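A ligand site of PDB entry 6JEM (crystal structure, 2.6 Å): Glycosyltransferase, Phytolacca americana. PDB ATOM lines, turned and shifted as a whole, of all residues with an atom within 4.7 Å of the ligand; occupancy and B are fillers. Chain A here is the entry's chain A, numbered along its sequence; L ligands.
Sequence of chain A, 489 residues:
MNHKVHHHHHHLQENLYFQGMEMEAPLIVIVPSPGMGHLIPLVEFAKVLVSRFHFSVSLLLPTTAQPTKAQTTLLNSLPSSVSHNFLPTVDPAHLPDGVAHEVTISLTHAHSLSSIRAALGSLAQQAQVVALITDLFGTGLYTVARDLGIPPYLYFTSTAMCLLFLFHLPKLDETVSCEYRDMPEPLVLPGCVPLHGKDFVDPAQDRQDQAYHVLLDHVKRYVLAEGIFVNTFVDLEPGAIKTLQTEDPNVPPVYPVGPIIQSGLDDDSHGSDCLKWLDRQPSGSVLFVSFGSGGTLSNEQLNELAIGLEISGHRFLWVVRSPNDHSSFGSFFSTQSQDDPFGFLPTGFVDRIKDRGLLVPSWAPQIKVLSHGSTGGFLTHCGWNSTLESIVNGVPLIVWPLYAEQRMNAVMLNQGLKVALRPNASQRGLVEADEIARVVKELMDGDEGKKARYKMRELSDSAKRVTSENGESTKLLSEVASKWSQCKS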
ATOM      1  N   GLY A  37     -11.186   2.146 -20.915  1.00  0.00           N
ATOM      2  CA  GLY A  37      -9.989   1.781 -21.693  1.00  0.00           C
ATOM      3  C   GLY A  37      -8.740   1.709 -20.825  1.00  0.00           C
ATOM      4  O   GLY A  37      -7.650   1.317 -21.349  1.00  0.00           O
ATOM      5  N   PRO A  41      -8.046  -3.390 -19.758  1.00  0.00           N
ATOM      6  CA  PRO A  41      -6.720  -4.008 -19.809  1.00  0.00           C
ATOM      7  C   PRO A  41      -6.220  -4.448 -18.430  1.00  0.00           C
ATOM      8  O   PRO A  41      -5.665  -5.520 -18.340  1.00  0.00           O
ATOM      9  CB  PRO A  41      -5.809  -2.909 -20.389  1.00  0.00           C
ATOM     10  CG  PRO A  41      -6.757  -1.926 -21.057  1.00  0.00           C
ATOM     11  CD  PRO A  41      -8.068  -2.024 -20.301  1.00  0.00           C
ATOM     12  N   THR A 157      -0.167  -0.069 -21.208  1.00  0.00           N
ATOM     13  CA  THR A 157      -1.205  -0.740 -22.028  1.00  0.00           C
ATOM     14  C   THR A 157      -1.016  -0.460 -23.515  1.00  0.00           C
ATOM     15  O   THR A 157      -1.822  -0.958 -24.274  1.00  0.00           O
ATOM     16  CB  THR A 157      -2.590  -0.338 -21.538  1.00  0.00           C
ATOM     17  OG1 THR A 157      -2.676   1.090 -21.454  1.00  0.00           O
ATOM     18  CG2 THR A 157      -2.880  -0.947 -20.183  1.00  0.00           C
ATOM     19  N   SER A 158       0.004   0.305 -23.895  1.00  0.00           N
ATOM     20  CA  SER A 158       0.339   0.639 -25.302  1.00  0.00           C
ATOM     21  C   SER A 158       1.696   0.020 -25.687  1.00  0.00           C
ATOM     22  O   SER A 158       2.128  -0.924 -25.036  1.00  0.00           O
ATOM     23  CB  SER A 158       0.306   2.137 -25.497  1.00  0.00           C
ATOM     24  OG  SER A 158       0.393   2.456 -26.890  1.00  0.00           O
ATOM     25  N   GLN A 262      -8.618 -10.072 -24.250  1.00  0.00           N
ATOM     26  CA  GLN A 262      -9.912 -10.714 -23.860  1.00  0.00           C
ATOM     27  C   GLN A 262     -10.046 -12.029 -24.641  1.00  0.00           C
ATOM     28  O   GLN A 262      -9.577 -12.068 -25.814  1.00  0.00           O
ATOM     29  CB  GLN A 262     -11.109  -9.794 -24.136  1.00  0.00           C
ATOM     30  CG  GLN A 262     -10.994  -8.408 -23.496  1.00  0.00           C
ATOM     31  CD  GLN A 262     -12.274  -7.603 -23.472  1.00  0.00           C
ATOM     32  OE1 GLN A 262     -13.154  -7.810 -22.619  1.00  0.00           O
ATOM     33  NE2 GLN A 262     -12.374  -6.630 -24.363  1.00  0.00           N
ATOM     34  N   SER A 290     -14.414  -1.446 -37.866  1.00  0.00           N
ATOM     35  CA  SER A 290     -14.769  -1.037 -36.471  1.00  0.00           C
ATOM     36  C   SER A 290     -13.825   0.033 -35.950  1.00  0.00           C
ATOM     37  O   SER A 290     -12.608  -0.197 -35.877  1.00  0.00           O
ATOM     38  CB  SER A 290     -14.804  -2.166 -35.525  1.00  0.00           C
ATOM     39  OG  SER A 290     -15.330  -1.702 -34.287  1.00  0.00           O
ATOM     40  N   VAL A 319     -19.491  -2.308 -38.094  1.00  0.00           N
ATOM     41  CA  VAL A 319     -20.121  -1.824 -36.845  1.00  0.00           C
ATOM     42  C   VAL A 319     -20.364  -0.327 -37.006  1.00  0.00           C
ATOM     43  O   VAL A 319     -19.420   0.452 -36.985  1.00  0.00           O
ATOM     44  CB  VAL A 319     -19.261  -2.143 -35.622  1.00  0.00           C
ATOM     45  CG1 VAL A 319     -19.922  -1.663 -34.373  1.00  0.00           C
ATOM     46  CG2 VAL A 319     -18.934  -3.630 -35.560  1.00  0.00           C
ATOM     47  N   SER A 362     -23.905  -0.501 -33.237  1.00  0.00           N
ATOM     48  CA  SER A 362     -23.269  -0.293 -31.909  1.00  0.00           C
ATOM     49  C   SER A 362     -22.132  -1.289 -31.614  1.00  0.00           C
ATOM     50  O   SER A 362     -21.092  -0.810 -31.189  1.00  0.00           O
ATOM     51  CB  SER A 362     -24.310  -0.299 -30.830  1.00  0.00           C
ATOM     52  OG  SER A 362     -25.145   0.846 -30.980  1.00  0.00           O
ATOM     53  N   TRP A 363     -22.321  -2.602 -31.760  1.00  0.00           N
ATOM     54  CA  TRP A 363     -21.416  -3.600 -31.098  1.00  0.00           C
ATOM     55  C   TRP A 363     -21.353  -4.914 -31.889  1.00  0.00           C
ATOM     56  O   TRP A 363     -22.388  -5.341 -32.378  1.00  0.00           O
ATOM     57  CB  TRP A 363     -21.837  -3.873 -29.644  1.00  0.00           C
ATOM     58  CG  TRP A 363     -20.815  -4.640 -28.865  1.00  0.00           C
ATOM     59  CD1 TRP A 363     -19.740  -4.142 -28.190  1.00  0.00           C
ATOM     60  CD2 TRP A 363     -20.762  -6.076 -28.687  1.00  0.00           C
ATOM     61  NE1 TRP A 363     -19.017  -5.157 -27.608  1.00  0.00           N
ATOM     62  CE2 TRP A 363     -19.619  -6.348 -27.888  1.00  0.00           C
ATOM     63  CE3 TRP A 363     -21.555  -7.142 -29.129  1.00  0.00           C
ATOM     64  CZ2 TRP A 363     -19.252  -7.655 -27.537  1.00  0.00           C
ATOM     65  CZ3 TRP A 363     -21.207  -8.431 -28.762  1.00  0.00           C
ATOM     66  CH2 TRP A 363     -20.069  -8.674 -27.973  1.00  0.00           C
ATOM     67  N   ALA A 364     -20.166  -5.516 -31.970  1.00  0.00           N
ATOM     68  CA  ALA A 364     -19.942  -6.859 -32.559  1.00  0.00           C
ATOM     69  C   ALA A 364     -19.025  -7.649 -31.652  1.00  0.00           C
ATOM     70  O   ALA A 364     -18.213  -7.078 -30.948  1.00  0.00           O
ATOM     71  CB  ALA A 364     -19.350  -6.720 -33.950  1.00  0.00           C
ATOM     72  N   GLN A 366     -15.916  -8.706 -31.406  1.00  0.00           N
ATOM     73  CA  GLN A 366     -14.647  -8.442 -32.140  1.00  0.00           C
ATOM     74  C   GLN A 366     -13.767  -9.689 -32.181  1.00  0.00           C
ATOM     75  O   GLN A 366     -13.302 -10.052 -33.275  1.00  0.00           O
ATOM     76  CB  GLN A 366     -13.866  -7.259 -31.559  1.00  0.00           C
ATOM     77  CG  GLN A 366     -13.229  -6.398 -32.627  1.00  0.00           C
ATOM     78  CD  GLN A 366     -12.485  -5.166 -32.182  1.00  0.00           C
ATOM     79  OE1 GLN A 366     -12.962  -4.005 -32.297  1.00  0.00           O
ATOM     80  NE2 GLN A 366     -11.264  -5.413 -31.732  1.00  0.00           N
ATOM     81  N   ILE A 367     -13.473 -10.335 -31.060  1.00  0.00           N
ATOM     82  CA  ILE A 367     -12.466 -11.449 -31.121  1.00  0.00           C
ATOM     83  C   ILE A 367     -13.031 -12.584 -31.969  1.00  0.00           C
ATOM     84  O   ILE A 367     -12.266 -13.216 -32.704  1.00  0.00           O
ATOM     85  CB  ILE A 367     -11.973 -11.909 -29.740  1.00  0.00           C
ATOM     86  CG1 ILE A 367     -11.219 -10.802 -29.003  1.00  0.00           C
ATOM     87  CG2 ILE A 367     -11.066 -13.111 -29.915  1.00  0.00           C
ATOM     88  CD1 ILE A 367     -12.087  -9.944 -28.082  1.00  0.00           C
ATOM     89  N   HIS A 381      -9.181   1.838 -35.838  1.00  0.00           N
ATOM     90  CA  HIS A 381      -8.659   3.128 -35.345  1.00  0.00           C
ATOM     91  C   HIS A 381      -7.300   2.940 -34.667  1.00  0.00           C
ATOM     92  O   HIS A 381      -6.781   3.968 -34.170  1.00  0.00           O
ATOM     93  CB  HIS A 381      -9.672   3.821 -34.439  1.00  0.00           C
ATOM     94  CG  HIS A 381      -9.860   3.182 -33.106  1.00  0.00           C
ATOM     95  ND1 HIS A 381     -10.016   1.836 -32.958  1.00  0.00           N
ATOM     96  CD2 HIS A 381      -9.951   3.710 -31.868  1.00  0.00           C
ATOM     97  CE1 HIS A 381     -10.144   1.556 -31.679  1.00  0.00           C
ATOM     98  NE2 HIS A 381     -10.143   2.678 -30.990  1.00  0.00           N
ATOM     99  N   CYS A 382      -6.764   1.717 -34.621  1.00  0.00           N
ATOM    100  CA  CYS A 382      -5.385   1.404 -34.126  1.00  0.00           C
ATOM    101  C   CYS A 382      -5.201   1.553 -32.614  1.00  0.00           C
ATOM    102  O   CYS A 382      -4.044   1.601 -32.169  1.00  0.00           O
ATOM    103  CB  CYS A 382      -4.352   2.364 -34.669  1.00  0.00           C
ATOM    104  SG  CYS A 382      -4.252   2.320 -36.449  1.00  0.00           S
ATOM    105  N   GLY A 383      -6.271   1.580 -31.851  1.00  0.00           N
ATOM    106  CA  GLY A 383      -6.158   1.251 -30.426  1.00  0.00           C
ATOM    107  C   GLY A 383      -5.360  -0.009 -30.263  1.00  0.00           C
ATOM    108  O   GLY A 383      -5.510  -0.942 -31.096  1.00  0.00           O
ATOM    109  N   TRP A 384      -4.507  -0.064 -29.240  1.00  0.00           N
ATOM    110  CA  TRP A 384      -3.529  -1.154 -29.082  1.00  0.00           C
ATOM    111  C   TRP A 384      -4.214  -2.486 -28.801  1.00  0.00           C
ATOM    112  O   TRP A 384      -3.692  -3.499 -29.267  1.00  0.00           O
ATOM    113  CB  TRP A 384      -2.479  -0.798 -28.031  1.00  0.00           C
ATOM    114  CG  TRP A 384      -1.336  -1.757 -28.073  1.00  0.00           C
ATOM    115  CD1 TRP A 384      -0.912  -2.559 -27.065  1.00  0.00           C
ATOM    116  CD2 TRP A 384      -0.578  -2.109 -29.238  1.00  0.00           C
ATOM    117  NE1 TRP A 384       0.122  -3.329 -27.526  1.00  0.00           N
ATOM    118  CE2 TRP A 384       0.345  -3.079 -28.845  1.00  0.00           C
ATOM    119  CE3 TRP A 384      -0.527  -1.624 -30.559  1.00  0.00           C
ATOM    120  CZ2 TRP A 384       1.300  -3.608 -29.713  1.00  0.00           C
ATOM    121  CZ3 TRP A 384       0.417  -2.144 -31.423  1.00  0.00           C
ATOM    122  CH2 TRP A 384       1.298  -3.149 -31.006  1.00  0.00           C
ATOM    123  N   ASN A 385      -5.335  -2.504 -28.084  1.00  0.00           N
ATOM    124  CA  ASN A 385      -5.999  -3.785 -27.716  1.00  0.00           C
ATOM    125  C   ASN A 385      -6.595  -4.392 -28.989  1.00  0.00           C
ATOM    126  O   ASN A 385      -6.401  -5.615 -29.225  1.00  0.00           O
ATOM    127  CB  ASN A 385      -6.990  -3.637 -26.560  1.00  0.00           C
ATOM    128  CG  ASN A 385      -6.318  -3.203 -25.276  1.00  0.00           C
ATOM    129  OD1 ASN A 385      -6.294  -2.001 -24.952  1.00  0.00           O
ATOM    130  ND2 ASN A 385      -5.764  -4.177 -24.547  1.00  0.00           N
ATOM    131  N   SER A 386      -7.221  -3.574 -29.830  1.00  0.00           N
ATOM    132  CA  SER A 386      -7.766  -3.995 -31.143  1.00  0.00           C
ATOM    133  C   SER A 386      -6.606  -4.483 -32.013  1.00  0.00           C
ATOM    134  O   SER A 386      -6.703  -5.547 -32.588  1.00  0.00           O
ATOM    135  CB  SER A 386      -8.526  -2.882 -31.809  1.00  0.00           C
ATOM    136  OG  SER A 386      -9.819  -2.784 -31.228  1.00  0.00           O
ATOM    137  N   GLU A 389      -5.375  -7.950 -30.891  1.00  0.00           N
ATOM    138  CA  GLU A 389      -6.384  -8.980 -31.235  1.00  0.00           C
ATOM    139  C   GLU A 389      -6.176  -9.392 -32.699  1.00  0.00           C
ATOM    140  O   GLU A 389      -6.144 -10.599 -33.010  1.00  0.00           O
ATOM    141  CB  GLU A 389      -7.793  -8.454 -30.979  1.00  0.00           C
ATOM    142  CG  GLU A 389      -8.030  -8.258 -29.483  1.00  0.00           C
ATOM    143  CD  GLU A 389      -9.290  -7.539 -29.056  1.00  0.00           C
ATOM    144  OE1 GLU A 389     -10.147  -7.246 -29.975  1.00  0.00           O
ATOM    145  OE2 GLU A 389      -9.425  -7.357 -27.811  1.00  0.00           O
ATOM    146  N   TYR A 403      -7.197   9.243 -32.172  1.00  0.00           N
ATOM    147  CA  TYR A 403      -6.856   9.936 -30.914  1.00  0.00           C
ATOM    148  C   TYR A 403      -5.810   9.171 -30.090  1.00  0.00           C
ATOM    149  O   TYR A 403      -5.294   8.116 -30.522  1.00  0.00           O
ATOM    150  CB  TYR A 403      -8.130  10.243 -30.101  1.00  0.00           C
ATOM    151  CG  TYR A 403      -8.869   9.052 -29.605  1.00  0.00           C
ATOM    152  CD1 TYR A 403      -9.867   8.474 -30.367  1.00  0.00           C
ATOM    153  CD2 TYR A 403      -8.599   8.501 -28.363  1.00  0.00           C
ATOM    154  CE1 TYR A 403     -10.556   7.339 -29.929  1.00  0.00           C
ATOM    155  CE2 TYR A 403      -9.301   7.395 -27.891  1.00  0.00           C
ATOM    156  CZ  TYR A 403     -10.258   6.792 -28.696  1.00  0.00           C
ATOM    157  OH  TYR A 403     -10.921   5.690 -28.267  1.00  0.00           O
ATOM    158  N   ALA A 404      -5.434   9.759 -28.957  1.00  0.00           N
ATOM    159  CA  ALA A 404      -4.407   9.231 -28.014  1.00  0.00           C
ATOM    160  C   ALA A 404      -3.102   8.956 -28.785  1.00  0.00           C
ATOM    161  O   ALA A 404      -2.592   9.875 -29.395  1.00  0.00           O
ATOM    162  CB  ALA A 404      -4.972   8.014 -27.342  1.00  0.00           C
ATOM    163  N   GLU A 405      -2.572   7.733 -28.759  1.00  0.00           N
ATOM    164  CA  GLU A 405      -1.284   7.373 -29.377  1.00  0.00           C
ATOM    165  C   GLU A 405      -1.548   6.630 -30.711  1.00  0.00           C
ATOM    166  O   GLU A 405      -0.600   6.003 -31.261  1.00  0.00           O
ATOM    167  CB  GLU A 405      -0.450   6.563 -28.371  1.00  0.00           C
ATOM    168  CG  GLU A 405      -0.594   5.052 -28.476  1.00  0.00           C
ATOM    169  CD  GLU A 405      -1.889   4.458 -27.939  1.00  0.00           C
ATOM    170  OE1 GLU A 405      -1.904   3.224 -27.670  1.00  0.00           O
ATOM    171  OE2 GLU A 405      -2.868   5.210 -27.779  1.00  0.00           O
ATOM    172  N   GLN A 406      -2.756   6.740 -31.267  1.00  0.00           N
ATOM    173  CA  GLN A 406      -3.173   5.927 -32.438  1.00  0.00           C
ATOM    174  C   GLN A 406      -2.370   6.345 -33.667  1.00  0.00           C
ATOM    175  O   GLN A 406      -2.009   5.442 -34.440  1.00  0.00           O
ATOM    176  CB  GLN A 406      -4.681   6.050 -32.638  1.00  0.00           C
ATOM    177  CG  GLN A 406      -5.469   5.295 -31.578  1.00  0.00           C
ATOM    178  CD  GLN A 406      -6.890   5.752 -31.485  1.00  0.00           C
ATOM    179  OE1 GLN A 406      -7.437   6.349 -32.421  1.00  0.00           O
ATOM    180  NE2 GLN A 406      -7.482   5.508 -30.333  1.00  0.00           N
ATOM    181  N   ASN A 409       0.765   4.579 -33.547  1.00  0.00           N
ATOM    182  CA  ASN A 409       0.543   3.114 -33.785  1.00  0.00           C
ATOM    183  C   ASN A 409       0.442   2.893 -35.291  1.00  0.00           C
ATOM    184  O   ASN A 409       1.034   1.917 -35.790  1.00  0.00           O
ATOM    185  CB  ASN A 409      -0.666   2.594 -33.014  1.00  0.00           C
ATOM    186  CG  ASN A 409      -0.453   2.554 -31.509  1.00  0.00           C
ATOM    187  OD1 ASN A 409       0.698   2.611 -31.041  1.00  0.00           O
ATOM    188  ND2 ASN A 409      -1.543   2.429 -30.759  1.00  0.00           N
HETATM  189  C1  LIG L   1      -7.646   2.636 -25.389  1.00  0.00           C
HETATM  190  O1  LIG L   1      -8.285   1.517 -25.962  1.00  0.00           O
HETATM  191  P1  LIG L   1      -9.865   1.462 -26.181  1.00  0.00           P
HETATM  192  O2  LIG L   1     -10.393   2.849 -26.315  1.00  0.00           O
HETATM  193  O3  LIG L   1     -10.474   0.585 -25.132  1.00  0.00           O
HETATM  194  O4  LIG L   1      -9.965   0.717 -27.597  1.00  0.00           O
HETATM  195  P2  LIG L   1      -9.271  -0.598 -28.187  1.00  0.00           P
HETATM  196  O5  LIG L   1      -7.832  -0.601 -27.798  1.00  0.00           O
HETATM  197  O6  LIG L   1      -9.608  -0.714 -29.641  1.00  0.00           O
HETATM  198  O7  LIG L   1     -10.051  -1.749 -27.375  1.00  0.00           O
HETATM  199  C2  LIG L   1     -11.346  -2.182 -27.857  1.00  0.00           C
HETATM  200  C3  LIG L   1     -11.807  -3.372 -27.049  1.00  0.00           C
HETATM  201  O8  LIG L   1     -13.250  -3.486 -27.122  1.00  0.00           O
HETATM  202  C4  LIG L   1     -13.611  -4.654 -27.834  1.00  0.00           C
HETATM  203  C5  LIG L   1     -12.346  -5.176 -28.516  1.00  0.00           C
HETATM  204  C6  LIG L   1     -11.275  -4.746 -27.504  1.00  0.00           C
HETATM  205  O9  LIG L   1     -11.184  -5.644 -26.412  1.00  0.00           O
HETATM  206  O10 LIG L   1     -12.431  -6.579 -28.662  1.00  0.00           O
HETATM  207  N1  LIG L   1     -14.675  -4.321 -28.794  1.00  0.00           N
HETATM  208  C7  LIG L   1     -15.652  -5.270 -29.013  1.00  0.00           C
HETATM  209  O11 LIG L   1     -15.665  -6.358 -28.452  1.00  0.00           O
HETATM  210  N2  LIG L   1     -16.628  -4.908 -29.917  1.00  0.00           N
HETATM  211  C8  LIG L   1     -16.710  -3.706 -30.607  1.00  0.00           C
HETATM  212  O12 LIG L   1     -17.647  -3.534 -31.385  1.00  0.00           O
HETATM  213  C9  LIG L   1     -15.658  -2.781 -30.328  1.00  0.00           C
HETATM  214  C10 LIG L   1     -14.696  -3.103 -29.451  1.00  0.00           C
HETATM  215  C11 LIG L   1      -7.363   3.632 -26.494  1.00  0.00           C
HETATM  216  F1  LIG L   1      -8.556   3.877 -27.193  1.00  0.00           F
HETATM  217  C12 LIG L   1      -6.325   3.114 -27.462  1.00  0.00           C
HETATM  218  O13 LIG L   1      -5.976   4.153 -28.379  1.00  0.00           O
HETATM  219  C13 LIG L   1      -5.096   2.660 -26.688  1.00  0.00           C
HETATM  220  O14 LIG L   1      -4.153   2.060 -27.583  1.00  0.00           O
HETATM  221  C14 LIG L   1      -5.485   1.643 -25.622  1.00  0.00           C
HETATM  222  C15 LIG L   1      -4.327   1.191 -24.774  1.00  0.00           C
HETATM  223  O15 LIG L   1      -4.772   0.519 -23.601  1.00  0.00           O
HETATM  224  O16 LIG L   1      -6.453   2.241 -24.740  1.00  0.00           O
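The side-chain amide nitrogen (ND2) of Asn 409 sits at hydrogen-bond distance from the side-chain carboxylate (OE1) of Glu 405, at 3.2 Å. N of Tyr 403 is in hydrogen-bond range of OE1 of Gln 406 (2.9 Å). OG of Ser 386 lies within hydrogen-bond range of NE2 of Gln 366. OE1 of Glu 389 sits at hydrogen-bond distance from NE2 of Gln 366 (2.8 Å). The backbone carbonyl oxygen (O) of His 381 lies close to the side-chain amide oxygen (OE1) of Gln 406 (3.0 Å). OG of Ser 158 is in hydrogen-bond range of OE1 of Glu 405, 2.5 Å away.
The indole nitrogen of Trp 363 lies close to a nitrogen (N2) of the ligand. Merely in contact with the ligand: His 381 (3.1 Å), Ile 367 (3.4 Å), Gly 383 (3.5 Å) and Gly 37 (3.7 Å). Hydrophobic or aromatic side chains within 4 Å of the ligand: Trp 363, Ile 367, His 381, Trp 384 and Tyr 403. Within 4 Å of the ligand: Gly 37, Thr 157, Gln 262, Trp 363, Ala 364, Gln 366, Ile 367, His 381, Gly 383, Trp 384, Asn 385, Ser 386, Glu 389, Tyr 403, Glu 405 and Gln 406. The nearest printed residue that does not touch the ligand is Pro 41 (4.05 Å).
The backbone NH (N) of Asn 385 sits at hydrogen-bond distance from an oxygen (O5) of the ligand (3.2 Å). The side-chain carboxylate of Glu 389 lies within hydrogen-bond range of an oxygen (O10) of the ligand (2.7 Å). OE1 of Glu 405 sits at hydrogen-bond distance from O14 of the ligand, 2.5 Å away. O2 of the ligand is in hydrogen-bond range of OH of Tyr 403, 3.5 Å away. The backbone carbonyl oxygen of Thr 157 sits close to an oxygen (O15) of the ligand, at 3.4 Å. O9 of the ligand sits at hydrogen-bond distance from NE2 of Gln 262 (2.6 Å). The side-chain hydroxyl (OG) of Ser 386 is in hydrogen-bond range of an oxygen (O6) of the ligand (2.6 Å). The side-chain hydroxyl (OG1) of Thr 157 lies within hydrogen-bond range of an oxygen (O15) of the ligand (3.1 Å). N2 of the ligand lies within hydrogen-bond range of O of Ala 364. The side-chain amide nitrogen (NE2) of Gln 366 lies close to an oxygen (O10) of the ligand (3.5 Å). The backbone NH (N) of Trp 384 is in hydrogen-bond range of an oxygen (O14) of the ligand (2.7 Å). O15 of the ligand lies within hydrogen-bond range of OD1 of Asn 385 (3.2 Å). N of Ala 364 lies within hydrogen-bond range of O12 of the ligand. An oxygen (O13) of the ligand is in hydrogen-bond range of the side-chain amide nitrogen (NE2) of Gln 406.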
